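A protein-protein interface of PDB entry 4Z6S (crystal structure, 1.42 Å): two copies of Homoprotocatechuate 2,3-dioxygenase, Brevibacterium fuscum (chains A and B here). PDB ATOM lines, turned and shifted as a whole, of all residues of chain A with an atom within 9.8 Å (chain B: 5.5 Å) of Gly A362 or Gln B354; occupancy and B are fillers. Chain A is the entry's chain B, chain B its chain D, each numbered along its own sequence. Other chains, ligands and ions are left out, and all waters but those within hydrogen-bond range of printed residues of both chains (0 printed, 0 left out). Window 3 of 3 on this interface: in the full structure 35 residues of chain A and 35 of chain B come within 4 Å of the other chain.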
ATOM      1  N   VAL A 300     -17.754   2.754 -23.361  1.00  0.00           N
ATOM      2  CA  VAL A 300     -16.860   1.929 -22.526  1.00  0.00           C
ATOM      3  C   VAL A 300     -16.665   2.630 -21.195  1.00  0.00           C
ATOM      4  O   VAL A 300     -16.225   3.801 -21.116  1.00  0.00           O
ATOM      5  CB  VAL A 300     -15.509   1.667 -23.232  1.00  0.00           C
ATOM      6  CG1 VAL A 300     -14.611   0.806 -22.374  1.00  0.00           C
ATOM      7  CG2 VAL A 300     -15.738   0.978 -24.569  1.00  0.00           C
ATOM      8  N   VAL A 301     -17.017   1.912 -20.132  1.00  0.00           N
ATOM      9  CA  VAL A 301     -16.932   2.457 -18.789  1.00  0.00           C
ATOM     10  C   VAL A 301     -15.475   2.800 -18.465  1.00  0.00           C
ATOM     11  O   VAL A 301     -14.576   2.008 -18.774  1.00  0.00           O
ATOM     12  CB  VAL A 301     -17.534   1.480 -17.740  1.00  0.00           C
ATOM     13  CG1 VAL A 301     -18.972   1.112 -18.109  1.00  0.00           C
ATOM     14  CG2 VAL A 301     -16.709   0.251 -17.578  1.00  0.00           C
ATOM     15  N   PRO A 302     -15.238   3.969 -17.814  1.00  0.00           N
ATOM     16  CA  PRO A 302     -13.845   4.417 -17.657  1.00  0.00           C
ATOM     17  C   PRO A 302     -12.975   3.448 -16.856  1.00  0.00           C
ATOM     18  O   PRO A 302     -11.758   3.308 -17.144  1.00  0.00           O
ATOM     19  CB  PRO A 302     -13.946   5.776 -16.980  1.00  0.00           C
ATOM     20  CG  PRO A 302     -15.389   6.136 -16.985  1.00  0.00           C
ATOM     21  CD  PRO A 302     -16.223   5.012 -17.488  1.00  0.00           C
ATOM     22  N   SER A 303     -13.575   2.772 -15.873  1.00  0.00           N
ATOM     23  CA  SER A 303     -12.809   1.826 -15.076  1.00  0.00           C
ATOM     24  C   SER A 303     -12.251   0.686 -15.913  1.00  0.00           C
ATOM     25  O   SER A 303     -11.230   0.062 -15.533  1.00  0.00           O
ATOM     26  CB  SER A 303     -13.644   1.259 -13.939  1.00  0.00           C
ATOM     27  OG  SER A 303     -14.748   0.526 -14.429  1.00  0.00           O
ATOM     28  N   THR A 306      -8.878   1.947 -16.775  1.00  0.00           N
ATOM     29  CA  THR A 306      -7.969   2.386 -15.729  1.00  0.00           C
ATOM     30  C   THR A 306      -7.634   1.296 -14.699  1.00  0.00           C
ATOM     31  O   THR A 306      -6.556   1.328 -14.084  1.00  0.00           O
ATOM     32  CB  THR A 306      -8.471   3.647 -14.996  1.00  0.00           C
ATOM     33  OG1 THR A 306      -9.683   3.360 -14.311  1.00  0.00           O
ATOM     34  CG2 THR A 306      -8.710   4.790 -15.977  1.00  0.00           C
ATOM     35  N   LEU A 330      -8.612   5.684 -23.544  1.00  0.00           N
ATOM     36  CA  LEU A 330      -9.611   6.492 -22.855  1.00  0.00           C
ATOM     37  C   LEU A 330      -9.544   7.943 -23.317  1.00  0.00           C
ATOM     38  O   LEU A 330     -10.549   8.531 -23.724  1.00  0.00           O
ATOM     39  CB  LEU A 330      -9.382   6.403 -21.359  1.00  0.00           C
ATOM     40  CG  LEU A 330     -10.407   7.134 -20.477  1.00  0.00           C
ATOM     41  CD1 LEU A 330     -10.390   6.494 -19.106  1.00  0.00           C
ATOM     42  CD2 LEU A 330     -10.107   8.623 -20.372  1.00  0.00           C
ATOM     43  N   ILE A 334     -12.908   9.079 -25.237  1.00  0.00           N
ATOM     44  CA  ILE A 334     -13.985   9.558 -24.337  1.00  0.00           C
ATOM     45  C   ILE A 334     -13.550  10.648 -23.376  1.00  0.00           C
ATOM     46  O   ILE A 334     -14.388  11.182 -22.630  1.00  0.00           O
ATOM     47  CB  ILE A 334     -14.672   8.418 -23.567  1.00  0.00           C
ATOM     48  CG1 ILE A 334     -13.700   7.701 -22.634  1.00  0.00           C
ATOM     49  CG2 ILE A 334     -15.341   7.477 -24.542  1.00  0.00           C
ATOM     50  CD1 ILE A 334     -14.345   6.659 -21.723  1.00  0.00           C
ATOM     51  N   GLY A 335     -12.260  11.005 -23.408  1.00  0.00           N
ATOM     52  CA  GLY A 335     -11.762  12.112 -22.609  1.00  0.00           C
ATOM     53  C   GLY A 335     -12.125  13.453 -23.219  1.00  0.00           C
ATOM     54  O   GLY A 335     -12.791  13.533 -24.266  1.00  0.00           O
ATOM     55  N   GLY A 353     -15.278  15.063 -27.179  1.00  0.00           N
ATOM     56  CA  GLY A 353     -14.976  15.336 -25.767  1.00  0.00           C
ATOM     57  C   GLY A 353     -15.934  14.707 -24.780  1.00  0.00           C
ATOM     58  O   GLY A 353     -16.099  15.191 -23.641  1.00  0.00           O
ATOM     59  N   GLN A 354     -16.594  13.634 -25.205  1.00  0.00           N
ATOM     60  CA  GLN A 354     -17.390  12.883 -24.294  1.00  0.00           C
ATOM     61  C   GLN A 354     -17.692  11.505 -24.823  1.00  0.00           C
ATOM     62  O   GLN A 354     -17.269  11.154 -25.928  1.00  0.00           O
ATOM     63  CB  GLN A 354     -18.663  13.629 -23.935  1.00  0.00           C
ATOM     64  CG  GLN A 354     -19.749  13.733 -24.963  1.00  0.00           C
ATOM     65  CD  GLN A 354     -21.013  14.313 -24.302  1.00  0.00           C
ATOM     66  OE1 GLN A 354     -20.968  15.419 -23.743  1.00  0.00           O
ATOM     67  NE2 GLN A 354     -22.123  13.542 -24.298  1.00  0.00           N
ATOM     68  N   ALA A 355     -18.378  10.715 -24.010  1.00  0.00           N
ATOM     69  CA  ALA A 355     -18.756   9.380 -24.425  1.00  0.00           C
ATOM     70  C   ALA A 355     -20.033   9.394 -25.273  1.00  0.00           C
ATOM     71  O   ALA A 355     -20.736  10.420 -25.409  1.00  0.00           O
ATOM     72  CB  ALA A 355     -18.940   8.487 -23.210  1.00  0.00           C
ATOM     73  N   PHE A 359     -23.394  10.576 -22.221  1.00  0.00           N
ATOM     74  CA  PHE A 359     -22.592  10.555 -21.024  1.00  0.00           C
ATOM     75  C   PHE A 359     -21.233  11.239 -21.162  1.00  0.00           C
ATOM     76  O   PHE A 359     -20.687  11.338 -22.259  1.00  0.00           O
ATOM     77  CB  PHE A 359     -22.393   9.120 -20.563  1.00  0.00           C
ATOM     78  CG  PHE A 359     -23.672   8.418 -20.171  1.00  0.00           C
ATOM     79  CD1 PHE A 359     -24.443   8.874 -19.118  1.00  0.00           C
ATOM     80  CD2 PHE A 359     -24.113   7.310 -20.879  1.00  0.00           C
ATOM     81  CE1 PHE A 359     -25.618   8.209 -18.750  1.00  0.00           C
ATOM     82  CE2 PHE A 359     -25.282   6.670 -20.528  1.00  0.00           C
ATOM     83  CZ  PHE A 359     -26.034   7.119 -19.464  1.00  0.00           C
ATOM     84  N   LYS A 360     -20.709  11.707 -20.022  1.00  0.00           N
ATOM     85  CA  LYS A 360     -19.334  12.167 -19.880  1.00  0.00           C
ATOM     86  C   LYS A 360     -18.669  11.339 -18.798  1.00  0.00           C
ATOM     87  O   LYS A 360     -19.353  10.621 -18.058  1.00  0.00           O
ATOM     88  CB  LYS A 360     -19.304  13.662 -19.453  1.00  0.00           C
ATOM     89  CG  LYS A 360     -19.099  14.618 -20.601  1.00  0.00           C
ATOM     90  CD  LYS A 360     -19.122  16.072 -20.119  1.00  0.00           C
ATOM     91  CE  LYS A 360     -18.769  17.018 -21.265  1.00  0.00           C
ATOM     92  NZ  LYS A 360     -19.272  18.410 -21.070  1.00  0.00           N
ATOM     93  N   LEU A 361     -17.344  11.422 -18.719  1.00  0.00           N
ATOM     94  CA  LEU A 361     -16.572  10.767 -17.644  1.00  0.00           C
ATOM     95  C   LEU A 361     -17.008  11.273 -16.271  1.00  0.00           C
ATOM     96  O   LEU A 361     -17.062  12.484 -16.062  1.00  0.00           O
ATOM     97  CB  LEU A 361     -15.078  11.089 -17.787  1.00  0.00           C
ATOM     98  CG  LEU A 361     -14.261  10.574 -18.971  1.00  0.00           C
ATOM     99  CD1 LEU A 361     -12.851  11.163 -18.941  1.00  0.00           C
ATOM    100  CD2 LEU A 361     -14.185   9.068 -18.944  1.00  0.00           C
ATOM    101  N   GLY A 362     -17.267  10.356 -15.330  1.00  0.00           N
ATOM    102  CA  GLY A 362     -17.541  10.742 -13.940  1.00  0.00           C
ATOM    103  C   GLY A 362     -16.312  11.115 -13.116  1.00  0.00           C
ATOM    104  O   GLY A 362     -15.173  11.184 -13.603  1.00  0.00           O
ATOM    105  N   THR B 333     -31.968  11.460  -9.468  1.00  0.00           N
ATOM    106  CA  THR B 333     -31.208  10.191  -9.575  1.00  0.00           C
ATOM    107  C   THR B 333     -29.804  10.313 -10.183  1.00  0.00           C
ATOM    108  O   THR B 333     -28.856   9.710  -9.657  1.00  0.00           O
ATOM    109  CB  THR B 333     -32.002   9.100 -10.342  1.00  0.00           C
ATOM    110  OG1 THR B 333     -32.206   9.498 -11.696  1.00  0.00           O
ATOM    111  CG2 THR B 333     -33.353   8.828  -9.674  1.00  0.00           C
ATOM    112  N   ILE B 334     -29.673  11.087 -11.266  1.00  0.00           N
ATOM    113  CA  ILE B 334     -28.409  11.160 -12.021  1.00  0.00           C
ATOM    114  C   ILE B 334     -27.881  12.579 -12.222  1.00  0.00           C
ATOM    115  O   ILE B 334     -26.772  12.737 -12.760  1.00  0.00           O
ATOM    116  CB  ILE B 334     -28.492  10.410 -13.388  1.00  0.00           C
ATOM    117  CG1 ILE B 334     -29.543  11.027 -14.354  1.00  0.00           C
ATOM    118  CG2 ILE B 334     -28.756   8.932 -13.146  1.00  0.00           C
ATOM    119  CD1 ILE B 334     -29.528  10.479 -15.771  1.00  0.00           C
ATOM    120  N   GLY B 335     -28.651  13.586 -11.789  1.00  0.00           N
ATOM    121  CA  GLY B 335     -28.171  14.965 -11.780  1.00  0.00           C
ATOM    122  C   GLY B 335     -27.124  15.249 -10.707  1.00  0.00           C
ATOM    123  O   GLY B 335     -26.838  14.396  -9.871  1.00  0.00           O
ATOM    124  N   ALA B 336     -26.604  16.476 -10.692  1.00  0.00           N
ATOM    125  CA  ALA B 336     -25.537  16.853  -9.752  1.00  0.00           C
ATOM    126  C   ALA B 336     -25.914  16.677  -8.256  1.00  0.00           C
ATOM    127  O   ALA B 336     -25.031  16.432  -7.417  1.00  0.00           O
ATOM    128  CB  ALA B 336     -25.085  18.286 -10.030  1.00  0.00           C
ATOM    129  N   GLY B 338     -28.434  14.468  -7.409  1.00  0.00           N
ATOM    130  CA  GLY B 338     -29.155  13.193  -7.415  1.00  0.00           C
ATOM    131  C   GLY B 338     -28.384  12.108  -6.688  1.00  0.00           C
ATOM    132  O   GLY B 338     -27.203  12.255  -6.396  1.00  0.00           O
ATOM    133  N   SER B 340     -28.503   7.438  -6.437  1.00  0.00           N
ATOM    134  CA  SER B 340     -29.173   6.164  -6.520  1.00  0.00           C
ATOM    135  C   SER B 340     -28.372   5.137  -5.713  1.00  0.00           C
ATOM    136  O   SER B 340     -27.201   5.354  -5.372  1.00  0.00           O
ATOM    137  CB  SER B 340     -29.339   5.726  -7.978  1.00  0.00           C
ATOM    138  OG  SER B 340     -28.085   5.378  -8.569  1.00  0.00           O
ATOM    139  N   TYR B 351     -24.461   5.935  -5.816  1.00  0.00           N
ATOM    140  CA  TYR B 351     -23.973   6.924  -6.766  1.00  0.00           C
ATOM    141  C   TYR B 351     -24.537   8.263  -6.382  1.00  0.00           C
ATOM    142  O   TYR B 351     -25.733   8.382  -6.149  1.00  0.00           O
ATOM    143  CB  TYR B 351     -24.384   6.545  -8.194  1.00  0.00           C
ATOM    144  CG  TYR B 351     -23.976   5.154  -8.531  1.00  0.00           C
ATOM    145  CD1 TYR B 351     -22.639   4.852  -8.787  1.00  0.00           C
ATOM    146  CD2 TYR B 351     -24.892   4.118  -8.514  1.00  0.00           C
ATOM    147  CE1 TYR B 351     -22.240   3.557  -9.060  1.00  0.00           C
ATOM    148  CE2 TYR B 351     -24.504   2.822  -8.773  1.00  0.00           C
ATOM    149  CZ  TYR B 351     -23.172   2.540  -9.049  1.00  0.00           C
ATOM    150  OH  TYR B 351     -22.789   1.235  -9.320  1.00  0.00           O
ATOM    151  N   HIS B 352     -23.665   9.252  -6.223  1.00  0.00           N
ATOM    152  CA  HIS B 352     -24.061  10.592  -5.781  1.00  0.00           C
ATOM    153  C   HIS B 352     -23.558  11.622  -6.790  1.00  0.00           C
ATOM    154  O   HIS B 352     -22.351  11.737  -7.032  1.00  0.00           O
ATOM    155  CB  HIS B 352     -23.463  10.890  -4.406  1.00  0.00           C
ATOM    156  CG  HIS B 352     -23.885   9.913  -3.350  1.00  0.00           C
ATOM    157  ND1 HIS B 352     -25.020  10.085  -2.591  1.00  0.00           N
ATOM    158  CD2 HIS B 352     -23.358   8.726  -2.970  1.00  0.00           C
ATOM    159  CE1 HIS B 352     -25.171   9.053  -1.783  1.00  0.00           C
ATOM    160  NE2 HIS B 352     -24.168   8.220  -1.983  1.00  0.00           N
ATOM    161  N   GLY B 353     -24.489  12.353  -7.381  1.00  0.00           N
ATOM    162  CA  GLY B 353     -24.171  13.434  -8.301  1.00  0.00           C
ATOM    163  C   GLY B 353     -23.757  12.941  -9.664  1.00  0.00           C
ATOM    164  O   GLY B 353     -23.225  13.705 -10.481  1.00  0.00           O
ATOM    165  N   GLN B 354     -24.028  11.667  -9.925  1.00  0.00           N
ATOM    166  CA  GLN B 354     -23.700  11.083 -11.225  1.00  0.00           C
ATOM    167  C   GLN B 354     -24.447   9.803 -11.424  1.00  0.00           C
ATOM    168  O   GLN B 354     -25.125   9.318 -10.490  1.00  0.00           O
ATOM    169  CB  GLN B 354     -22.203  10.876 -11.402  1.00  0.00           C
ATOM    170  CG  GLN B 354     -21.525   9.832 -10.552  1.00  0.00           C
ATOM    171  CD  GLN B 354     -20.016   9.871 -10.803  1.00  0.00           C
ATOM    172  OE1 GLN B 354     -19.407  10.930 -10.732  1.00  0.00           O
ATOM    173  NE2 GLN B 354     -19.436   8.749 -11.175  1.00  0.00           N
ATOM    174  N   ALA B 355     -24.336   9.274 -12.641  1.00  0.00           N
ATOM    175  CA  ALA B 355     -24.993   8.030 -12.971  1.00  0.00           C
ATOM    176  C   ALA B 355     -24.139   6.831 -12.484  1.00  0.00           C
ATOM    177  O   ALA B 355     -23.046   6.979 -11.944  1.00  0.00           O
ATOM    178  CB  ALA B 355     -25.234   7.942 -14.467  1.00  0.00           C
ATOM    179  N   SER B 356     -24.678   5.636 -12.663  1.00  0.00           N
ATOM    180  CA  SER B 356     -23.968   4.417 -12.376  1.00  0.00           C
ATOM    181  C   SER B 356     -22.872   4.170 -13.412  1.00  0.00           C
ATOM    182  O   SER B 356     -22.821   4.826 -14.465  1.00  0.00           O
ATOM    183  CB  SER B 356     -24.963   3.251 -12.371  1.00  0.00           C
ATOM    184  OG  SER B 356     -25.669   3.218 -13.606  1.00  0.00           O
ATOM    185  N   GLY B 358     -19.797   4.760 -13.688  1.00  0.00           N
ATOM    186  CA  GLY B 358     -18.671   5.683 -13.861  1.00  0.00           C
ATOM    187  C   GLY B 358     -18.961   6.886 -14.728  1.00  0.00           C
ATOM    188  O   GLY B 358     -18.027   7.633 -15.078  1.00  0.00           O
ATOM    189  N   PHE B 359     -20.226   7.090 -15.094  1.00  0.00           N
ATOM    190  CA  PHE B 359     -20.588   8.190 -16.003  1.00  0.00           C
ATOM    191  C   PHE B 359     -21.277   9.330 -15.274  1.00  0.00           C
ATOM    192  O   PHE B 359     -21.982   9.105 -14.294  1.00  0.00           O
ATOM    193  CB  PHE B 359     -21.525   7.669 -17.093  1.00  0.00           C
ATOM    194  CG  PHE B 359     -20.903   6.621 -17.976  1.00  0.00           C
ATOM    195  CD1 PHE B 359     -19.833   6.951 -18.793  1.00  0.00           C
ATOM    196  CD2 PHE B 359     -21.394   5.320 -17.985  1.00  0.00           C
ATOM    197  CE1 PHE B 359     -19.248   6.001 -19.614  1.00  0.00           C
ATOM    198  CE2 PHE B 359     -20.808   4.352 -18.788  1.00  0.00           C
ATOM    199  CZ  PHE B 359     -19.733   4.700 -19.612  1.00  0.00           C
ATOM    200  N   LYS B 360     -21.094  10.544 -15.771  1.00  0.00           N
ATOM    201  CA  LYS B 360     -21.989  11.650 -15.437  1.00  0.00           C
ATOM    202  C   LYS B 360     -22.707  12.141 -16.689  1.00  0.00           C
ATOM    203  O   LYS B 360     -22.482  11.635 -17.785  1.00  0.00           O
ATOM    204  CB  LYS B 360     -21.220  12.780 -14.748  1.00  0.00           C
ATOM    205  CG  LYS B 360     -20.368  13.620 -15.653  1.00  0.00           C
ATOM    206  CD  LYS B 360     -19.654  14.735 -14.876  1.00  0.00           C
ATOM    207  CE  LYS B 360     -18.991  15.709 -15.841  1.00  0.00           C
ATOM    208  NZ  LYS B 360     -18.241  16.805 -15.151  1.00  0.00           N
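The backbone NH (N) of Lys A360 lies within hydrogen-bond range of the backbone carbonyl oxygen (O) of Lys B360 (2.9 Å).
The backbone carbonyl oxygen of Gly B358 is in hydrogen-bond range of the backbone NH of Gly A362 (2.8 Å).
O of Phe A359 lies within hydrogen-bond range of NE2 of Gln A354, 3.3 Å away.
Among the printed residues, merely in contact across the chains: Val A300 with Phe B359 (3.9 Å), Val A301 with Phe B359 (3.7 Å), Pro A302 with Gly B358 (3.6 Å), Pro A302 with Phe B359 (3.8 Å), Phe A359 with Phe B359 (3.8 Å), Phe A359 with Lys B360 (3.4 Å), Lys A360 with Phe B359 (3.4 Å), Leu A361 with Gly B358 (3.96 Å), Leu A361 with Lys B360 (3.5 Å), Gly A362 with Gln B354 (3.7 Å) and Gly A362 with Lys B360 (3.9 Å).
Of the printed residues of chain B, Val A301 touches Phe B359.
Printed residues of chain B within 4 Å of Lys A360: Phe B359 and Lys B360.
Of chain B, only Gln B354 (3.7 Å), Gly B358 (2.8 Å) and Lys B360 (3.9 Å) come within 4 Å of Gly A362.
Gly B335 touches none of the printed residues of chain A.
No residue of chain A comes within 4 Å of Gly B353.
Of chain A, only Gly A362 (3.7 Å) comes within 4 Å of Gln B354.
No residue of chain A comes within 4 Å of Ala B355.
Gly B358 touches three residues of chain A.
Printed residues of chain A within 4 Å of Phe B359: Val A300 (3.9 Å), Val A301 (3.7 Å), Pro A302 (3.8 Å), Phe A359 (3.8 Å) and Lys A360 (3.4 Å).
Of the 15 printed residues of chain A, 7 touch a printed residue of chain B.
Printed residues of chain A that touch a printed residue of chain B: Val A300, Val A301, Pro A302, Phe A359, Lys A360, Leu A361 and Gly A362.
Printed residues of chain B that touch a printed residue of chain A: Gln B354, Gly B358, Phe B359 and Lys B360.
Hydrophobic or aromatic side chains of chain B within 4 Å of the printed part of chain A: Phe B359.
Along chain B the printed residues that touch a printed residue of chain A span positions 354 to 360.
Among the printed residues, no Asp or Glu carboxylate lies within 4 Å of a Lys or Arg side-chain nitrogen of the other chain.
Phe A359 touches its own counterpart, Phe B359.
Phe A359 touches Lys B360, and with the chains exchanged Lys A360 touches Phe B359.
Lys B360 touches its own counterpart, Lys A360.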
